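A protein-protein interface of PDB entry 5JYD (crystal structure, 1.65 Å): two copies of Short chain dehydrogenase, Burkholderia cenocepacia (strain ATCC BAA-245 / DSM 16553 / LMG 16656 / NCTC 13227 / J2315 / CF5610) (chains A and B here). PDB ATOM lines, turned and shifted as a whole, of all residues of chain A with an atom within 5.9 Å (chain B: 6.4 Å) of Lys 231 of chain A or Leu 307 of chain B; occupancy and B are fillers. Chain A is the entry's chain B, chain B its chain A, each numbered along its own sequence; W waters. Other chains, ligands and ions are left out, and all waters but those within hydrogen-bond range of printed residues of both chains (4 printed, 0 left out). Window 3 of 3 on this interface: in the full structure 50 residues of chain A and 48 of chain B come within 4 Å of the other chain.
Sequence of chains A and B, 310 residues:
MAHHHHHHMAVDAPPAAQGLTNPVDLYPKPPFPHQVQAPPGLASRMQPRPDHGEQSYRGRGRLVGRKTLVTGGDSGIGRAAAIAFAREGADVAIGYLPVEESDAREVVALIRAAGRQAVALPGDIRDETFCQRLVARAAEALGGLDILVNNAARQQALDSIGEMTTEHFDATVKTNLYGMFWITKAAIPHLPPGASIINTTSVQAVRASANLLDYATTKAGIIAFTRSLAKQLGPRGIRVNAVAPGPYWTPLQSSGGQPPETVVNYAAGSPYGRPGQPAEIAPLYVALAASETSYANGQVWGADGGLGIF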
ATOM      1  N   THR A 226     -19.319  26.120  26.958  1.00  0.00           N
ATOM      2  CA  THR A 226     -19.177  27.404  26.265  1.00  0.00           C
ATOM      3  C   THR A 226     -18.822  27.198  24.795  1.00  0.00           C
ATOM      4  O   THR A 226     -19.404  27.831  23.908  1.00  0.00           O
ATOM      5  CB  THR A 226     -18.093  28.229  26.976  1.00  0.00           C
ATOM      6  OG1 THR A 226     -18.484  28.484  28.332  1.00  0.00           O
ATOM      7  CG2 THR A 226     -17.852  29.571  26.300  1.00  0.00           C
ATOM      8  N   ARG A 227     -17.812  26.376  24.526  1.00  0.00           N
ATOM      9  CA  ARG A 227     -17.341  26.200  23.152  1.00  0.00           C
ATOM     10  C   ARG A 227     -18.414  25.545  22.288  1.00  0.00           C
ATOM     11  O   ARG A 227     -18.678  25.992  21.154  1.00  0.00           O
ATOM     12  CB  ARG A 227     -16.031  25.384  23.160  1.00  0.00           C
ATOM     13  CG  ARG A 227     -14.836  26.123  23.731  1.00  0.00           C
ATOM     14  CD  ARG A 227     -13.650  25.205  23.941  1.00  0.00           C
ATOM     15  NE  ARG A 227     -12.436  25.977  24.204  1.00  0.00           N
ATOM     16  CZ  ARG A 227     -11.336  25.543  24.807  1.00  0.00           C
ATOM     17  NH1 ARG A 227     -11.232  24.302  25.291  1.00  0.00           N
ATOM     18  NH2 ARG A 227     -10.319  26.381  24.929  1.00  0.00           N
ATOM     19  N   SER A 228     -19.077  24.511  22.813  1.00  0.00           N
ATOM     20  CA  SER A 228     -20.107  23.840  22.040  1.00  0.00           C
ATOM     21  C   SER A 228     -21.287  24.781  21.771  1.00  0.00           C
ATOM     22  O   SER A 228     -21.793  24.864  20.642  1.00  0.00           O
ATOM     23  CB  SER A 228     -20.598  22.596  22.766  1.00  0.00           C
ATOM     24  OG  SER A 228     -21.781  22.084  22.180  1.00  0.00           O
ATOM     25  N   LEU A 229     -21.717  25.523  22.788  1.00  0.00           N
ATOM     26  CA  LEU A 229     -22.854  26.411  22.585  1.00  0.00           C
ATOM     27  C   LEU A 229     -22.504  27.578  21.658  1.00  0.00           C
ATOM     28  O   LEU A 229     -23.367  28.035  20.901  1.00  0.00           O
ATOM     29  CB  LEU A 229     -23.370  26.918  23.934  1.00  0.00           C
ATOM     30  CG  LEU A 229     -24.705  27.671  23.926  1.00  0.00           C
ATOM     31  CD1 LEU A 229     -25.881  26.802  23.525  1.00  0.00           C
ATOM     32  CD2 LEU A 229     -24.926  28.263  25.335  1.00  0.00           C
ATOM     33  N   ALA A 230     -21.259  28.069  21.696  1.00  0.00           N
ATOM     34  CA  ALA A 230     -20.835  29.086  20.734  1.00  0.00           C
ATOM     35  C   ALA A 230     -20.993  28.592  19.303  1.00  0.00           C
ATOM     36  O   ALA A 230     -21.344  29.369  18.404  1.00  0.00           O
ATOM     37  CB  ALA A 230     -19.381  29.493  21.012  1.00  0.00           C
ATOM     38  N   LYS A 231     -20.758  27.307  19.071  1.00  0.00           N
ATOM     39  CA  LYS A 231     -20.920  26.786  17.719  1.00  0.00           C
ATOM     40  C   LYS A 231     -22.392  26.641  17.367  1.00  0.00           C
ATOM     41  O   LYS A 231     -22.763  26.795  16.202  1.00  0.00           O
ATOM     42  CB  LYS A 231     -20.193  25.449  17.569  1.00  0.00           C
ATOM     43  CG  LYS A 231     -18.668  25.521  17.745  1.00  0.00           C
ATOM     44  CD  LYS A 231     -18.031  24.198  17.382  1.00  0.00           C
ATOM     45  CE  LYS A 231     -16.498  24.195  17.718  1.00  0.00           C
ATOM     46  NZ  LYS A 231     -16.212  24.174  19.194  1.00  0.00           N
ATOM     47  N   GLN A 232     -23.241  26.364  18.359  1.00  0.00           N
ATOM     48  CA  GLN A 232     -24.684  26.320  18.121  1.00  0.00           C
ATOM     49  C   GLN A 232     -25.238  27.701  17.808  1.00  0.00           C
ATOM     50  O   GLN A 232     -26.038  27.870  16.870  1.00  0.00           O
ATOM     51  CB  GLN A 232     -25.416  25.783  19.351  1.00  0.00           C
ATOM     52  CG  GLN A 232     -25.387  24.307  19.529  1.00  0.00           C
ATOM     53  CD  GLN A 232     -26.418  23.834  20.537  1.00  0.00           C
ATOM     54  OE1 GLN A 232     -27.370  24.550  20.876  1.00  0.00           O
ATOM     55  NE2 GLN A 232     -26.252  22.615  20.994  1.00  0.00           N
ATOM     56  N   LEU A 233     -24.864  28.696  18.616  1.00  0.00           N
ATOM     57  CA  LEU A 233     -25.554  29.987  18.609  1.00  0.00           C
ATOM     58  C   LEU A 233     -24.861  31.063  17.783  1.00  0.00           C
ATOM     59  O   LEU A 233     -25.524  32.023  17.362  1.00  0.00           O
ATOM     60  CB  LEU A 233     -25.727  30.504  20.043  1.00  0.00           C
ATOM     61  CG  LEU A 233     -26.540  29.619  20.980  1.00  0.00           C
ATOM     62  CD1 LEU A 233     -26.590  30.306  22.339  1.00  0.00           C
ATOM     63  CD2 LEU A 233     -27.945  29.329  20.431  1.00  0.00           C
ATOM     64  N   GLY A 234     -23.560  30.922  17.535  1.00  0.00           N
ATOM     65  CA  GLY A 234     -22.832  31.860  16.711  1.00  0.00           C
ATOM     66  C   GLY A 234     -23.483  32.117  15.369  1.00  0.00           C
ATOM     67  O   GLY A 234     -23.610  33.263  14.929  1.00  0.00           O
ATOM     68  N   PRO A 235     -23.895  31.052  14.674  1.00  0.00           N
ATOM     69  CA  PRO A 235     -24.574  31.237  13.378  1.00  0.00           C
ATOM     70  C   PRO A 235     -25.875  32.029  13.474  1.00  0.00           C
ATOM     71  O   PRO A 235     -26.342  32.577  12.467  1.00  0.00           O
ATOM     72  CB  PRO A 235     -24.828  29.793  12.905  1.00  0.00           C
ATOM     73  CG  PRO A 235     -23.801  28.967  13.606  1.00  0.00           C
ATOM     74  CD  PRO A 235     -23.632  29.631  14.962  1.00  0.00           C
ATOM     75  N   ASN A 297     -15.951  34.575  19.946  1.00  0.00           N
ATOM     76  CA  ASN A 297     -17.017  33.611  20.186  1.00  0.00           C
ATOM     77  C   ASN A 297     -16.395  32.259  20.501  1.00  0.00           C
ATOM     78  O   ASN A 297     -15.474  31.835  19.804  1.00  0.00           O
ATOM     79  CB  ASN A 297     -17.950  33.519  18.954  1.00  0.00           C
ATOM     80  CG  ASN A 297     -19.151  32.652  19.190  1.00  0.00           C
ATOM     81  OD1 ASN A 297     -19.686  32.609  20.283  1.00  0.00           O
ATOM     82  ND2 ASN A 297     -19.558  31.910  18.169  1.00  0.00           N
ATOM     83  N   GLY A 298     -16.890  31.609  21.553  1.00  0.00           N
ATOM     84  CA  GLY A 298     -16.266  30.389  22.049  1.00  0.00           C
ATOM     85  C   GLY A 298     -14.930  30.584  22.749  1.00  0.00           C
ATOM     86  O   GLY A 298     -14.185  29.601  22.895  1.00  0.00           O
ATOM     87  N   VAL B 203      -4.400  30.971  16.142  1.00  0.00           N
ATOM     88  CA  VAL B 203      -4.975  29.653  16.419  1.00  0.00           C
ATOM     89  C   VAL B 203      -4.101  28.551  15.831  1.00  0.00           C
ATOM     90  O   VAL B 203      -4.152  27.411  16.309  1.00  0.00           O
ATOM     91  CB  VAL B 203      -6.420  29.510  15.903  1.00  0.00           C
ATOM     92  CG1 VAL B 203      -7.352  30.484  16.602  1.00  0.00           C
ATOM     93  CG2 VAL B 203      -6.524  29.639  14.383  1.00  0.00           C
ATOM     94  N   ARG B 207      -3.941  24.545  16.133  1.00  0.00           N
ATOM     95  CA  ARG B 207      -4.583  23.905  14.976  1.00  0.00           C
ATOM     96  C   ARG B 207      -3.552  23.224  14.072  1.00  0.00           C
ATOM     97  O   ARG B 207      -3.835  22.173  13.469  1.00  0.00           O
ATOM     98  CB  ARG B 207      -5.376  24.944  14.201  1.00  0.00           C
ATOM     99  CG  ARG B 207      -5.831  24.525  12.845  1.00  0.00           C
ATOM    100  CD  ARG B 207      -6.700  25.602  12.241  1.00  0.00           C
ATOM    101  NE  ARG B 207      -8.095  25.252  12.389  1.00  0.00           N
ATOM    102  CZ  ARG B 207      -9.067  25.821  11.695  1.00  0.00           C
ATOM    103  NH1 ARG B 207      -8.787  26.785  10.818  1.00  0.00           N
ATOM    104  NH2 ARG B 207     -10.316  25.426  11.886  1.00  0.00           N
ATOM    105  N   GLY B 246      -8.213  33.870  14.913  1.00  0.00           N
ATOM    106  CA  GLY B 246      -8.537  32.910  13.891  1.00  0.00           C
ATOM    107  C   GLY B 246      -8.357  33.540  12.520  1.00  0.00           C
ATOM    108  O   GLY B 246      -7.513  34.423  12.339  1.00  0.00           O
ATOM    109  N   PRO B 247      -9.147  33.113  11.529  1.00  0.00           N
ATOM    110  CA  PRO B 247      -8.962  33.612  10.154  1.00  0.00           C
ATOM    111  C   PRO B 247      -9.476  35.032   9.952  1.00  0.00           C
ATOM    112  O   PRO B 247     -10.649  35.321  10.210  1.00  0.00           O
ATOM    113  CB  PRO B 247      -9.759  32.609   9.317  1.00  0.00           C
ATOM    114  CG  PRO B 247     -10.842  32.173  10.217  1.00  0.00           C
ATOM    115  CD  PRO B 247     -10.219  32.094  11.585  1.00  0.00           C
ATOM    116  N   GLY B 269     -16.395  27.629   5.955  1.00  0.00           N
ATOM    117  CA  GLY B 269     -16.853  26.557   6.808  1.00  0.00           C
ATOM    118  C   GLY B 269     -16.888  26.887   8.277  1.00  0.00           C
ATOM    119  O   GLY B 269     -17.165  25.992   9.081  1.00  0.00           O
ATOM    120  N   SER B 270     -16.610  28.133   8.651  1.00  0.00           N
ATOM    121  CA  SER B 270     -16.578  28.553  10.055  1.00  0.00           C
ATOM    122  C   SER B 270     -18.002  28.813  10.546  1.00  0.00           C
ATOM    123  O   SER B 270     -18.943  28.864   9.757  1.00  0.00           O
ATOM    124  CB  SER B 270     -15.697  29.789  10.197  1.00  0.00           C
ATOM    125  OG  SER B 270     -16.339  30.932   9.649  1.00  0.00           O
ATOM    126  N   PRO B 271     -18.201  28.971  11.860  1.00  0.00           N
ATOM    127  CA  PRO B 271     -19.572  29.162  12.370  1.00  0.00           C
ATOM    128  C   PRO B 271     -20.294  30.361  11.774  1.00  0.00           C
ATOM    129  O   PRO B 271     -21.497  30.269  11.505  1.00  0.00           O
ATOM    130  CB  PRO B 271     -19.359  29.307  13.882  1.00  0.00           C
ATOM    131  CG  PRO B 271     -18.126  28.452  14.135  1.00  0.00           C
ATOM    132  CD  PRO B 271     -17.234  28.725  12.946  1.00  0.00           C
ATOM    133  N   ASP B 304     -11.665  34.160  17.350  1.00  0.00           N
ATOM    134  CA  ASP B 304     -11.630  33.233  16.224  1.00  0.00           C
ATOM    135  C   ASP B 304     -13.029  32.928  15.677  1.00  0.00           C
ATOM    136  O   ASP B 304     -13.195  32.026  14.841  1.00  0.00           O
ATOM    137  CB  ASP B 304     -10.862  31.961  16.628  1.00  0.00           C
ATOM    138  CG  ASP B 304     -11.502  31.191  17.786  1.00  0.00           C
ATOM    139  OD1 ASP B 304     -12.754  31.098  17.841  1.00  0.00           O
ATOM    140  OD2 ASP B 304     -10.730  30.680  18.640  1.00  0.00           O
ATOM    141  N   GLY B 305     -14.038  33.669  16.098  1.00  0.00           N
ATOM    142  CA  GLY B 305     -15.331  33.545  15.458  1.00  0.00           C
ATOM    143  C   GLY B 305     -16.111  32.295  15.819  1.00  0.00           C
ATOM    144  O   GLY B 305     -17.097  31.989  15.153  1.00  0.00           O
ATOM    145  N   GLY B 306     -15.709  31.550  16.849  1.00  0.00           N
ATOM    146  CA  GLY B 306     -16.398  30.338  17.234  1.00  0.00           C
ATOM    147  C   GLY B 306     -15.635  29.044  16.998  1.00  0.00           C
ATOM    148  O   GLY B 306     -16.160  27.973  17.313  1.00  0.00           O
ATOM    149  N   LEU B 307     -14.426  29.106  16.450  1.00  0.00           N
ATOM    150  CA  LEU B 307     -13.590  27.913  16.459  1.00  0.00           C
ATOM    151  C   LEU B 307     -13.326  27.467  17.899  1.00  0.00           C
ATOM    152  O   LEU B 307     -13.139  26.270  18.155  1.00  0.00           O
ATOM    153  CB  LEU B 307     -12.274  28.178  15.714  1.00  0.00           C
ATOM    154  CG  LEU B 307     -12.358  28.552  14.232  1.00  0.00           C
ATOM    155  CD1 LEU B 307     -10.967  28.698  13.650  1.00  0.00           C
ATOM    156  CD2 LEU B 307     -13.157  27.516  13.429  1.00  0.00           C
ATOM    157  N   GLY B 308     -13.231  28.424  18.829  1.00  0.00           N
ATOM    158  CA  GLY B 308     -13.122  28.117  20.245  1.00  0.00           C
ATOM    159  C   GLY B 308     -11.801  27.494  20.634  1.00  0.00           C
ATOM    160  O   GLY B 308     -11.787  26.419  21.262  1.00  0.00           O
ATOM    161  N   ILE B 309     -10.706  28.166  20.267  1.00  0.00           N
ATOM    162  CA  ILE B 309      -9.339  27.677  20.523  1.00  0.00           C
ATOM    163  C   ILE B 309      -8.721  28.364  21.755  1.00  0.00           C
ATOM    164  O   ILE B 309      -8.302  27.673  22.695  1.00  0.00           O
ATOM    165  CB  ILE B 309      -8.467  27.860  19.268  1.00  0.00           C
ATOM    166  CG1 ILE B 309      -9.117  27.175  18.063  1.00  0.00           C
ATOM    167  CG2 ILE B 309      -7.104  27.274  19.483  1.00  0.00           C
ATOM    168  CD1 ILE B 309      -9.555  25.767  18.252  1.00  0.00           C
HETATM  169  O   HOH W   1     -13.633  24.056  20.205  1.00  0.00           O
HETATM  170  O   HOH W   2     -16.377  27.078  19.930  1.00  0.00           O
HETATM  171  O   HOH W   3      -7.613  27.592  25.460  1.00  0.00           O
HETATM  172  O   HOH W   4     -11.610  28.775  23.575  1.00  0.00           O
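Lys 231 of chain A touches just these residues of chain B: Gly 306 and Leu 307. Printed residues of chain B within 4 Å of Asn 297 of chain A: Asp 304, Gly 305 and Gly 306. Pro 247 of chain B touches none of the printed residues of chain A. Of the printed residues of chain A, Gly 306 of chain B touches Lys 231 and Asn 297. Printed residues of chain A within 4 Å of Gly 308 of chain B: Arg 227 and Gly 298.
N of Gly 306 of chain B is in hydrogen-bond range of OD1 of Asp 304 of chain B, 3.1 Å away. The side-chain carboxylate (OD1) of Asp 304 of chain B is in hydrogen-bond range of the backbone NH (N) of Leu 307 of chain B (2.9 Å). OD1 of Asp 304 of chain B sits at hydrogen-bond distance from N of Gly 308 of chain B. OD2 of Asp 304 of chain B is in hydrogen-bond range of N of Ile 309 of chain B. The backbone carbonyl oxygen of Ala 230 of chain A is in hydrogen-bond range of the side-chain amide nitrogen of Asn 297 of chain A, at 3.1 Å.
Of the 12 printed residues of chain A, 5 touch a printed residue of chain B. Hydrophobic or aromatic side chains of chain A within 4 Å of the printed part of chain B: Pro 235. Among the printed residues, no Asp or Glu carboxylate lies within 4 Å of a Lys or Arg side-chain nitrogen of the other chain.
Water W1 lies within hydrogen-bond range of NZ of Lys 231 of chain A, O of Leu 307 of chain B and O of Gly 308 of chain B. Water W2 lies within hydrogen-bond range of the backbone carbonyl oxygen (O) of Gly 306 of chain B, the backbone carbonyl oxygen (O) of Arg 227 of chain A and the side-chain amino group (NZ) of Lys 231 of chain A. Water W4 lies within hydrogen-bond range of O of Gly 298 of chain A, NE of Arg 227 of chain A, O of Gly 308 of chain B and N of Ile 309 of chain B. Water W3 lies within hydrogen-bond range of O of Ile 309 of chain B and NH2 of Arg 227 of chain A.
No position is printed for both chains. Of the 9 pairs that touch across the chains among the printed residues, none has its exchanged pair printed and touching as well.
N of Gly 306 of chain B sits at hydrogen-bond distance from O of Asn 297 of chain A (3.0 Å). The guanidinium group (NE) of Arg 227 of chain A is in hydrogen-bond range of the backbone carbonyl oxygen (O) of Gly 308 of chain B (3.0 Å). O of Ile 309 of chain B is in hydrogen-bond range of NH2 of Arg 227 of chain A (3.3 Å). OD1 of Asp 304 of chain B sits close to O of Asn 297 of chain A (3.4 Å).
Among the printed residues, merely in contact across the chains: Gly 298 of chain A with Gly 308 of chain B, Pro 235 of chain A with Pro 271 of chain B, Lys 231 of chain A with Gly 306 of chain B, Asn 297 of chain A with Gly 305 of chain B and Lys 231 of chain A with Leu 307 of chain B.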
